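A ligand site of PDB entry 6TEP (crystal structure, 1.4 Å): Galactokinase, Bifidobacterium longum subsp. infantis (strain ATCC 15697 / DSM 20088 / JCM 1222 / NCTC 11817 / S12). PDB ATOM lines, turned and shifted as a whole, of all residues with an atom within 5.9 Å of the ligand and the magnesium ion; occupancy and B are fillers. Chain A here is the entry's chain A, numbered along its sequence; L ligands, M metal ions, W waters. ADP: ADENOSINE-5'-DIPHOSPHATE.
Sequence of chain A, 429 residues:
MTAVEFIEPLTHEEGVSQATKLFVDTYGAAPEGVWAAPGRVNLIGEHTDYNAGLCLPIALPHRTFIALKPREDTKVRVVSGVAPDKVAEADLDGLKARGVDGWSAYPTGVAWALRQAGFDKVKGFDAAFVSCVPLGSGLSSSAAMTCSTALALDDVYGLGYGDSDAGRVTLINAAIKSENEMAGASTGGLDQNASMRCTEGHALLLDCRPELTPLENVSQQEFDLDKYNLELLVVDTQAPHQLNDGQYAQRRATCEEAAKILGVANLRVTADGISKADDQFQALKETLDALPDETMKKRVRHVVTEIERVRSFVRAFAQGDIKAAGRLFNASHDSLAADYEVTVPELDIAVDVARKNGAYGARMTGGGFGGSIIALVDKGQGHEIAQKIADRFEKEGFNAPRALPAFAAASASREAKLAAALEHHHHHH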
ATOM      1  N   THR A  64     -10.425 -18.277 -15.649  1.00  0.00           N
ATOM      2  CA  THR A  64     -11.238 -18.596 -14.459  1.00  0.00           C
ATOM      3  C   THR A  64     -10.433 -19.561 -13.567  1.00  0.00           C
ATOM      4  O   THR A  64     -10.007 -20.657 -14.038  1.00  0.00           O
ATOM      5  CB  THR A  64     -12.589 -19.165 -14.899  1.00  0.00           C
ATOM      6  OG1 THR A  64     -13.292 -18.119 -15.552  1.00  0.00           O
ATOM      7  CG2 THR A  64     -13.378 -19.696 -13.716  1.00  0.00           C
ATOM      8  N   SER A  80     -18.823 -17.831  -6.106  1.00  0.00           N
ATOM      9  CA  SER A  80     -18.066 -17.089  -7.121  1.00  0.00           C
ATOM     10  C   SER A  80     -17.849 -15.679  -6.617  1.00  0.00           C
ATOM     11  O   SER A  80     -18.743 -15.125  -5.964  1.00  0.00           O
ATOM     12  CB  SER A  80     -18.797 -17.081  -8.431  1.00  0.00           C
ATOM     13  OG  SER A  80     -18.355 -16.083  -9.300  1.00  0.00           O
ATOM     14  N   GLY A  81     -16.683 -15.150  -6.968  1.00  0.00           N
ATOM     15  CA  GLY A  81     -16.380 -13.760  -6.665  1.00  0.00           C
ATOM     16  C   GLY A  81     -17.376 -12.774  -7.228  1.00  0.00           C
ATOM     17  O   GLY A  81     -17.318 -11.621  -6.798  1.00  0.00           O
ATOM     18  N   VAL A  82     -18.175 -13.102  -8.227  1.00  0.00           N
ATOM     19  CA  VAL A  82     -19.222 -12.181  -8.727  1.00  0.00           C
ATOM     20  C   VAL A  82     -20.228 -11.902  -7.612  1.00  0.00           C
ATOM     21  O   VAL A  82     -20.816 -10.774  -7.611  1.00  0.00           O
ATOM     22  CB  VAL A  82     -19.907 -12.752  -9.982  1.00  0.00           C
ATOM     23  CG1 VAL A  82     -18.919 -13.043 -11.086  1.00  0.00           C
ATOM     24  CG2 VAL A  82     -20.704 -14.001  -9.682  1.00  0.00           C
ATOM     25  N   GLY A 102     -29.686 -21.615 -12.257  1.00  0.00           N
ATOM     26  CA  GLY A 102     -28.748 -20.491 -12.142  1.00  0.00           C
ATOM     27  C   GLY A 102     -27.340 -20.872 -12.585  1.00  0.00           C
ATOM     28  O   GLY A 102     -27.142 -21.987 -13.165  1.00  0.00           O
ATOM     29  N   TRP A 103     -26.351 -20.057 -12.228  1.00  0.00           N
ATOM     30  CA  TRP A 103     -24.962 -20.221 -12.693  1.00  0.00           C
ATOM     31  C   TRP A 103     -24.422 -21.598 -12.202  1.00  0.00           C
ATOM     32  O   TRP A 103     -23.519 -22.129 -12.868  1.00  0.00           O
ATOM     33  CB  TRP A 103     -24.138 -19.051 -12.201  1.00  0.00           C
ATOM     34  CG  TRP A 103     -23.821 -19.082 -10.744  1.00  0.00           C
ATOM     35  CD1 TRP A 103     -24.600 -18.627  -9.709  1.00  0.00           C
ATOM     36  CD2 TRP A 103     -22.625 -19.588 -10.153  1.00  0.00           C
ATOM     37  NE1 TRP A 103     -23.948 -18.788  -8.523  1.00  0.00           N
ATOM     38  CE2 TRP A 103     -22.746 -19.392  -8.744  1.00  0.00           C
ATOM     39  CE3 TRP A 103     -21.498 -20.232 -10.659  1.00  0.00           C
ATOM     40  CZ2 TRP A 103     -21.750 -19.808  -7.862  1.00  0.00           C
ATOM     41  CZ3 TRP A 103     -20.503 -20.595  -9.789  1.00  0.00           C
ATOM     42  CH2 TRP A 103     -20.642 -20.385  -8.410  1.00  0.00           C
ATOM     43  N   TYR A 106     -23.595 -24.834 -14.244  1.00  0.00           N
ATOM     44  CA  TYR A 106     -22.387 -25.064 -15.095  1.00  0.00           C
ATOM     45  C   TYR A 106     -21.396 -25.975 -14.390  1.00  0.00           C
ATOM     46  O   TYR A 106     -21.084 -27.044 -14.920  1.00  0.00           O
ATOM     47  CB  TYR A 106     -21.765 -23.745 -15.526  1.00  0.00           C
ATOM     48  CG  TYR A 106     -22.610 -22.991 -16.496  1.00  0.00           C
ATOM     49  CD1 TYR A 106     -22.524 -23.284 -17.830  1.00  0.00           C
ATOM     50  CD2 TYR A 106     -23.445 -21.950 -16.140  1.00  0.00           C
ATOM     51  CE1 TYR A 106     -23.252 -22.588 -18.793  1.00  0.00           C
ATOM     52  CE2 TYR A 106     -24.227 -21.283 -17.069  1.00  0.00           C
ATOM     53  CZ  TYR A 106     -24.066 -21.526 -18.431  1.00  0.00           C
ATOM     54  OH  TYR A 106     -24.877 -20.850 -19.306  1.00  0.00           O
ATOM     55  N   PHE A 129     -14.840 -19.936  -7.201  1.00  0.00           N
ATOM     56  CA  PHE A 129     -14.365 -19.385  -8.497  1.00  0.00           C
ATOM     57  C   PHE A 129     -14.025 -17.892  -8.351  1.00  0.00           C
ATOM     58  O   PHE A 129     -14.822 -17.124  -7.785  1.00  0.00           O
ATOM     59  CB  PHE A 129     -15.453 -19.487  -9.565  1.00  0.00           C
ATOM     60  CG  PHE A 129     -15.806 -20.885  -9.945  1.00  0.00           C
ATOM     61  CD1 PHE A 129     -15.125 -21.515 -10.990  1.00  0.00           C
ATOM     62  CD2 PHE A 129     -16.801 -21.544  -9.256  1.00  0.00           C
ATOM     63  CE1 PHE A 129     -15.439 -22.832 -11.307  1.00  0.00           C
ATOM     64  CE2 PHE A 129     -17.098 -22.852  -9.561  1.00  0.00           C
ATOM     65  CZ  PHE A 129     -16.443 -23.484 -10.599  1.00  0.00           C
ATOM     66  N   VAL A 130     -12.882 -17.536  -8.973  1.00  0.00           N
ATOM     67  CA  VAL A 130     -12.500 -16.122  -9.204  1.00  0.00           C
ATOM     68  C   VAL A 130     -12.064 -16.069 -10.675  1.00  0.00           C
ATOM     69  O   VAL A 130     -11.328 -16.958 -11.103  1.00  0.00           O
ATOM     70  CB  VAL A 130     -11.350 -15.712  -8.293  1.00  0.00           C
ATOM     71  CG1 VAL A 130     -10.881 -14.323  -8.644  1.00  0.00           C
ATOM     72  CG2 VAL A 130     -11.748 -15.707  -6.800  1.00  0.00           C
ATOM     73  N   SER A 131     -12.586 -15.092 -11.416  1.00  0.00           N
ATOM     74  CA  SER A 131     -12.320 -14.959 -12.861  1.00  0.00           C
ATOM     75  C   SER A 131     -11.997 -13.533 -13.275  1.00  0.00           C
ATOM     76  O   SER A 131     -12.424 -12.542 -12.628  1.00  0.00           O
ATOM     77  CB  SER A 131     -13.492 -15.484 -13.599  1.00  0.00           C
ATOM     78  OG  SER A 131     -13.197 -15.547 -14.975  1.00  0.00           O
ATOM     79  N   VAL A 133     -12.334 -13.408 -16.825  1.00  0.00           N
ATOM     80  CA  VAL A 133     -13.131 -13.537 -18.072  1.00  0.00           C
ATOM     81  C   VAL A 133     -14.467 -12.869 -17.890  1.00  0.00           C
ATOM     82  O   VAL A 133     -15.318 -13.332 -17.126  1.00  0.00           O
ATOM     83  CB  VAL A 133     -13.317 -14.994 -18.534  1.00  0.00           C
ATOM     84  CG1 VAL A 133     -13.977 -15.001 -19.912  1.00  0.00           C
ATOM     85  CG2 VAL A 133     -11.989 -15.710 -18.520  1.00  0.00           C
ATOM     86  N   PRO A 134     -14.772 -11.790 -18.639  1.00  0.00           N
ATOM     87  CA  PRO A 134     -16.050 -11.123 -18.436  1.00  0.00           C
ATOM     88  C   PRO A 134     -17.216 -12.070 -18.781  1.00  0.00           C
ATOM     89  O   PRO A 134     -17.134 -12.887 -19.715  1.00  0.00           O
ATOM     90  CB  PRO A 134     -15.987  -9.873 -19.315  1.00  0.00           C
ATOM     91  CG  PRO A 134     -14.658  -9.900 -20.030  1.00  0.00           C
ATOM     92  CD  PRO A 134     -13.964 -11.199 -19.704  1.00  0.00           C
ATOM     93  N   LEU A 135     -18.295 -11.976 -17.993  1.00  0.00           N
ATOM     94  CA  LEU A 135     -19.539 -12.783 -18.177  1.00  0.00           C
ATOM     95  C   LEU A 135     -20.361 -12.216 -19.338  1.00  0.00           C
ATOM     96  O   LEU A 135     -20.792 -11.088 -19.248  1.00  0.00           O
ATOM     97  CB  LEU A 135     -20.376 -12.767 -16.883  1.00  0.00           C
ATOM     98  CG  LEU A 135     -19.942 -13.690 -15.748  1.00  0.00           C
ATOM     99  CD1 LEU A 135     -18.593 -13.326 -15.143  1.00  0.00           C
ATOM    100  CD2 LEU A 135     -21.040 -13.690 -14.686  1.00  0.00           C
ATOM    101  N   GLY A 136     -20.758 -13.084 -20.260  1.00  0.00           N
ATOM    102  CA  GLY A 136     -21.768 -12.746 -21.272  1.00  0.00           C
ATOM    103  C   GLY A 136     -21.257 -11.790 -22.333  1.00  0.00           C
ATOM    104  O   GLY A 136     -22.112 -11.246 -23.062  1.00  0.00           O
ATOM    105  N   SER A 137     -19.936 -11.764 -22.528  1.00  0.00           N
ATOM    106  CA  SER A 137     -19.242 -10.835 -23.469  1.00  0.00           C
ATOM    107  C   SER A 137     -18.776 -11.553 -24.736  1.00  0.00           C
ATOM    108  O   SER A 137     -18.175 -10.864 -25.559  1.00  0.00           O
ATOM    109  CB  SER A 137     -18.068 -10.186 -22.844  1.00  0.00           C
ATOM    110  OG  SER A 137     -18.461  -9.355 -21.780  1.00  0.00           O
ATOM    111  N   GLY A 138     -19.132 -12.844 -24.931  1.00  0.00           N
ATOM    112  CA  GLY A 138     -18.775 -13.643 -26.114  1.00  0.00           C
ATOM    113  C   GLY A 138     -17.329 -14.125 -26.078  1.00  0.00           C
ATOM    114  O   GLY A 138     -16.769 -14.431 -27.135  1.00  0.00           O
ATOM    115  N   LEU A 139     -16.744 -14.188 -24.885  1.00  0.00           N
ATOM    116  CA  LEU A 139     -15.350 -14.584 -24.662  1.00  0.00           C
ATOM    117  C   LEU A 139     -15.318 -15.936 -23.927  1.00  0.00           C
ATOM    118  O   LEU A 139     -14.242 -16.363 -23.503  1.00  0.00           O
ATOM    119  CB  LEU A 139     -14.621 -13.480 -23.899  1.00  0.00           C
ATOM    120  CG  LEU A 139     -14.585 -12.150 -24.612  1.00  0.00           C
ATOM    121  CD1 LEU A 139     -13.873 -11.141 -23.727  1.00  0.00           C
ATOM    122  CD2 LEU A 139     -13.920 -12.267 -26.002  1.00  0.00           C
ATOM    123  N   SER A 140     -16.479 -16.569 -23.723  1.00  0.00           N
ATOM    124  CA  SER A 140     -16.519 -17.977 -23.239  1.00  0.00           C
ATOM    125  C   SER A 140     -16.255 -18.091 -21.737  1.00  0.00           C
ATOM    126  O   SER A 140     -15.548 -19.058 -21.333  1.00  0.00           O
ATOM    127  CB  SER A 140     -15.573 -18.837 -24.045  1.00  0.00           C
ATOM    128  OG  SER A 140     -15.804 -18.662 -25.433  1.00  0.00           O
ATOM    129  N   SER A 141     -16.858 -17.212 -20.909  1.00  0.00           N
ATOM    130  CA  SER A 141     -16.804 -17.437 -19.455  1.00  0.00           C
ATOM    131  C   SER A 141     -17.408 -18.805 -19.188  1.00  0.00           C
ATOM    132  O   SER A 141     -16.926 -19.446 -18.188  1.00  0.00           O
ATOM    133  CB  SER A 141     -17.464 -16.326 -18.681  1.00  0.00           C
ATOM    134  OG  SER A 141     -18.864 -16.266 -18.851  1.00  0.00           O
ATOM    135  N   SER A 142     -18.421 -19.193 -19.971  1.00  0.00           N
ATOM    136  CA  SER A 142     -19.129 -20.508 -19.738  1.00  0.00           C
ATOM    137  C   SER A 142     -18.155 -21.696 -19.885  1.00  0.00           C
ATOM    138  O   SER A 142     -18.040 -22.504 -18.987  1.00  0.00           O
ATOM    139  CB  SER A 142     -20.327 -20.648 -20.631  1.00  0.00           C
ATOM    140  OG  SER A 142     -19.941 -20.430 -22.013  1.00  0.00           O
ATOM    141  N   ALA A 143     -17.312 -21.740 -20.925  1.00  0.00           N
ATOM    142  CA  ALA A 143     -16.320 -22.829 -21.052  1.00  0.00           C
ATOM    143  C   ALA A 143     -15.222 -22.713 -19.999  1.00  0.00           C
ATOM    144  O   ALA A 143     -14.714 -23.711 -19.527  1.00  0.00           O
ATOM    145  CB  ALA A 143     -15.717 -22.850 -22.421  1.00  0.00           C
ATOM    146  N   MET A 145     -15.536 -21.753 -17.088  1.00  0.00           N
ATOM    147  CA  MET A 145     -16.095 -22.320 -15.830  1.00  0.00           C
ATOM    148  C   MET A 145     -16.210 -23.859 -15.954  1.00  0.00           C
ATOM    149  O   MET A 145     -15.816 -24.537 -15.047  1.00  0.00           O
ATOM    150  CB  MET A 145     -17.477 -21.719 -15.572  1.00  0.00           C
ATOM    151  CG  MET A 145     -18.183 -22.281 -14.420  1.00  0.00           C
ATOM    152  SD  MET A 145     -19.393 -21.168 -13.664  1.00  0.00           S
ATOM    153  CE  MET A 145     -18.349 -20.037 -12.764  1.00  0.00           C
ATOM    154  N   GLU A 179     -23.214 -27.873 -20.023  1.00  0.00           N
ATOM    155  CA  GLU A 179     -23.800 -26.617 -20.530  1.00  0.00           C
ATOM    156  C   GLU A 179     -25.074 -26.907 -21.346  1.00  0.00           C
ATOM    157  O   GLU A 179     -25.988 -26.216 -21.201  1.00  0.00           O
ATOM    158  CB  GLU A 179     -22.799 -25.933 -21.456  1.00  0.00           C
ATOM    159  CG  GLU A 179     -23.363 -24.681 -22.045  1.00  0.00           C
ATOM    160  CD  GLU A 179     -22.310 -23.690 -22.489  1.00  0.00           C
ATOM    161  OE1 GLU A 179     -21.129 -24.023 -22.431  1.00  0.00           O
ATOM    162  OE2 GLU A 179     -22.721 -22.685 -22.928  1.00  0.00           O
ATOM    163  N   ALA A 185     -28.046 -24.505 -22.303  1.00  0.00           N
ATOM    164  CA  ALA A 185     -27.466 -23.582 -23.286  1.00  0.00           C
ATOM    165  C   ALA A 185     -26.834 -24.417 -24.391  1.00  0.00           C
ATOM    166  O   ALA A 185     -25.865 -25.084 -24.114  1.00  0.00           O
ATOM    167  CB  ALA A 185     -26.397 -22.739 -22.632  1.00  0.00           C
ATOM    168  N   ASP A 191     -15.578 -23.733 -28.018  1.00  0.00           N
ATOM    169  CA  ASP A 191     -15.117 -22.966 -26.871  1.00  0.00           C
ATOM    170  C   ASP A 191     -14.364 -23.851 -25.875  1.00  0.00           C
ATOM    171  O   ASP A 191     -13.315 -23.514 -25.352  1.00  0.00           O
ATOM    172  CB  ASP A 191     -16.331 -22.397 -26.092  1.00  0.00           C
ATOM    173  CG  ASP A 191     -17.289 -21.506 -26.841  1.00  0.00           C
ATOM    174  OD1 ASP A 191     -16.954 -21.061 -27.935  1.00  0.00           O
ATOM    175  OD2 ASP A 191     -18.376 -21.216 -26.283  1.00  0.00           O
HETATM  176  PB  ADP L   1     -20.130 -16.202 -22.320  1.00  0.00           P
HETATM  177  O1B ADP L   1     -19.287 -15.527 -21.256  1.00  0.00           O
HETATM  178  O2B ADP L   1     -19.753 -17.642 -22.494  1.00  0.00           O
HETATM  179  O3B ADP L   1     -20.120 -15.437 -23.658  1.00  0.00           O
HETATM  180  PA  ADP L   1     -22.608 -17.357 -21.406  1.00  0.00           P
HETATM  181  O1A ADP L   1     -22.510 -18.611 -22.236  1.00  0.00           O
HETATM  182  O2A ADP L   1     -23.993 -16.836 -21.318  1.00  0.00           O
HETATM  183  O3A ADP L   1     -21.660 -16.187 -21.907  1.00  0.00           O
HETATM  184  O5' ADP L   1     -22.007 -17.731 -19.967  1.00  0.00           O
HETATM  185  C5' ADP L   1     -22.121 -16.789 -18.897  1.00  0.00           C
HETATM  186  C4' ADP L   1     -22.859 -17.442 -17.759  1.00  0.00           C
HETATM  187  O4' ADP L   1     -22.002 -18.438 -17.172  1.00  0.00           O
HETATM  188  C3' ADP L   1     -23.178 -16.455 -16.643  1.00  0.00           C
HETATM  189  O3' ADP L   1     -24.422 -15.838 -16.864  1.00  0.00           O
HETATM  190  C2' ADP L   1     -23.204 -17.392 -15.421  1.00  0.00           C
HETATM  191  O2' ADP L   1     -24.397 -18.110 -15.418  1.00  0.00           O
HETATM  192  C1' ADP L   1     -22.020 -18.288 -15.772  1.00  0.00           C
HETATM  193  N9  ADP L   1     -20.743 -17.741 -15.344  1.00  0.00           N
HETATM  194  C8  ADP L   1     -19.623 -17.557 -16.132  1.00  0.00           C
HETATM  195  N7  ADP L   1     -18.597 -17.095 -15.467  1.00  0.00           N
HETATM  196  C5  ADP L   1     -19.044 -17.031 -14.129  1.00  0.00           C
HETATM  197  C6  ADP L   1     -18.418 -16.625 -12.931  1.00  0.00           C
HETATM  198  N6  ADP L   1     -17.168 -16.191 -12.822  1.00  0.00           N
HETATM  199  N1  ADP L   1     -19.160 -16.710 -11.779  1.00  0.00           N
HETATM  200  C2  ADP L   1     -20.417 -17.121 -11.852  1.00  0.00           C
HETATM  201  N3  ADP L   1     -21.121 -17.484 -12.922  1.00  0.00           N
HETATM  202  C4  ADP L   1     -20.348 -17.432 -14.051  1.00  0.00           C
HETATM  203 MG    MG M   1     -20.848 -19.126 -23.532  1.00  0.00          MG
HETATM  204  O   HOH W   1     -21.642 -17.885 -25.013  1.00  0.00           O
HETATM  205  O   HOH W   2     -21.707 -20.706 -24.283  1.00  0.00           O
HETATM  206  O   HOH W   3     -15.907 -18.505 -15.977  1.00  0.00           O
HETATM  207  O   HOH W   4     -18.847 -16.848 -25.563  1.00  0.00           O
HETATM  208  O   HOH W   5     -24.014 -20.725 -21.712  1.00  0.00           O
HETATM  209  O   HOH W   6     -17.610 -13.592 -22.199  1.00  0.00           O
HETATM  210  O   HOH W   7     -26.670 -17.077 -14.402  1.00  0.00           O
HETATM  211  O   HOH W   8     -15.683 -15.301 -10.405  1.00  0.00           O
HETATM  212  O   HOH W   9     -19.308 -19.172 -24.799  1.00  0.00           O
HETATM  213  O   HOH W  10     -16.271 -15.554 -15.497  1.00  0.00           O
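An oxygen (O1B) of the ligand is in hydrogen-bond range of the backbone NH (N) of Gly 136. The backbone NH (N) of Ser 141 sits at hydrogen-bond distance from an oxygen (O1B) of the ligand (3.0 Å). The backbone NH of Ser 142 sits close to an oxygen (O2B) of the ligand (3.2 Å). The side-chain hydroxyl of Ser 80 sits at hydrogen-bond distance from a nitrogen (N1) of the ligand (2.7 Å). The backbone NH (N) of Gly 138 lies within hydrogen-bond range of an oxygen (O3B) of the ligand (3.1 Å). The side-chain hydroxyl of Ser 141 is in hydrogen-bond range of an oxygen (O1B) of the ligand (2.6 Å).
The side-chain hydroxyl of Ser 80 lies close to the backbone NH of Val 82, 3.2 Å away. OG of Ser 131 lies within hydrogen-bond range of OG1 of Thr 64. OG of Ser 131 lies within hydrogen-bond range of N of Val 133 (3.0 Å).
The magnesium ion is bound by water W2 (1.9 Å), water W9 (2.0 Å), water W1 (2.1 Å), an oxygen (O2B) of the ligand (2.1 Å), an oxygen (O1A) of the ligand (2.2 Å) and the side-chain hydroxyl (OG) of Ser 142 (2.2 Å).
Merely in contact with the ligand: Ser 140 (3.3 Å), Trp 103 (3.4 Å), Met 145 (3.4 Å), Tyr 106 (3.6 Å), Leu 135 (3.7 Å), Pro 134 (3.7 Å), Val 82 (3.7 Å), Leu 139 (3.8 Å), Ser 131 (3.8 Å) and Ser 137 (3.8 Å).
Of the 25 residues printed, 1 comes within 4 Å of the magnesium ion. The nearest printed residue that does not touch the magnesium ion is Glu 179 (4.1 Å).
Water W5 bridges the side-chain hydroxyl of Tyr 106 (2.6 Å) and the side-chain carboxylate of Glu 179 (2.6 Å). Water W4 lies within hydrogen-bond range of an oxygen (O3B) of the ligand (2.7 Å), the backbone NH of Ser 140 (3.0 Å) and the backbone NH of Leu 139 (3.5 Å). Water W10 lies within hydrogen-bond range of N7 of the ligand, O of Val 133 and OG of Ser 131. Water W8 lies within hydrogen-bond range of a nitrogen (N6) of the ligand, the side-chain hydroxyl of Ser 80, the backbone NH of Ser 131 and the backbone carbonyl oxygen of Phe 129. Water W3 lies within hydrogen-bond range of O of Ser 141 (2.6 Å), OG1 of Thr 64 (2.7 Å), N7 of the ligand (3.1 Å) and N of Met 145 (3.5 Å).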
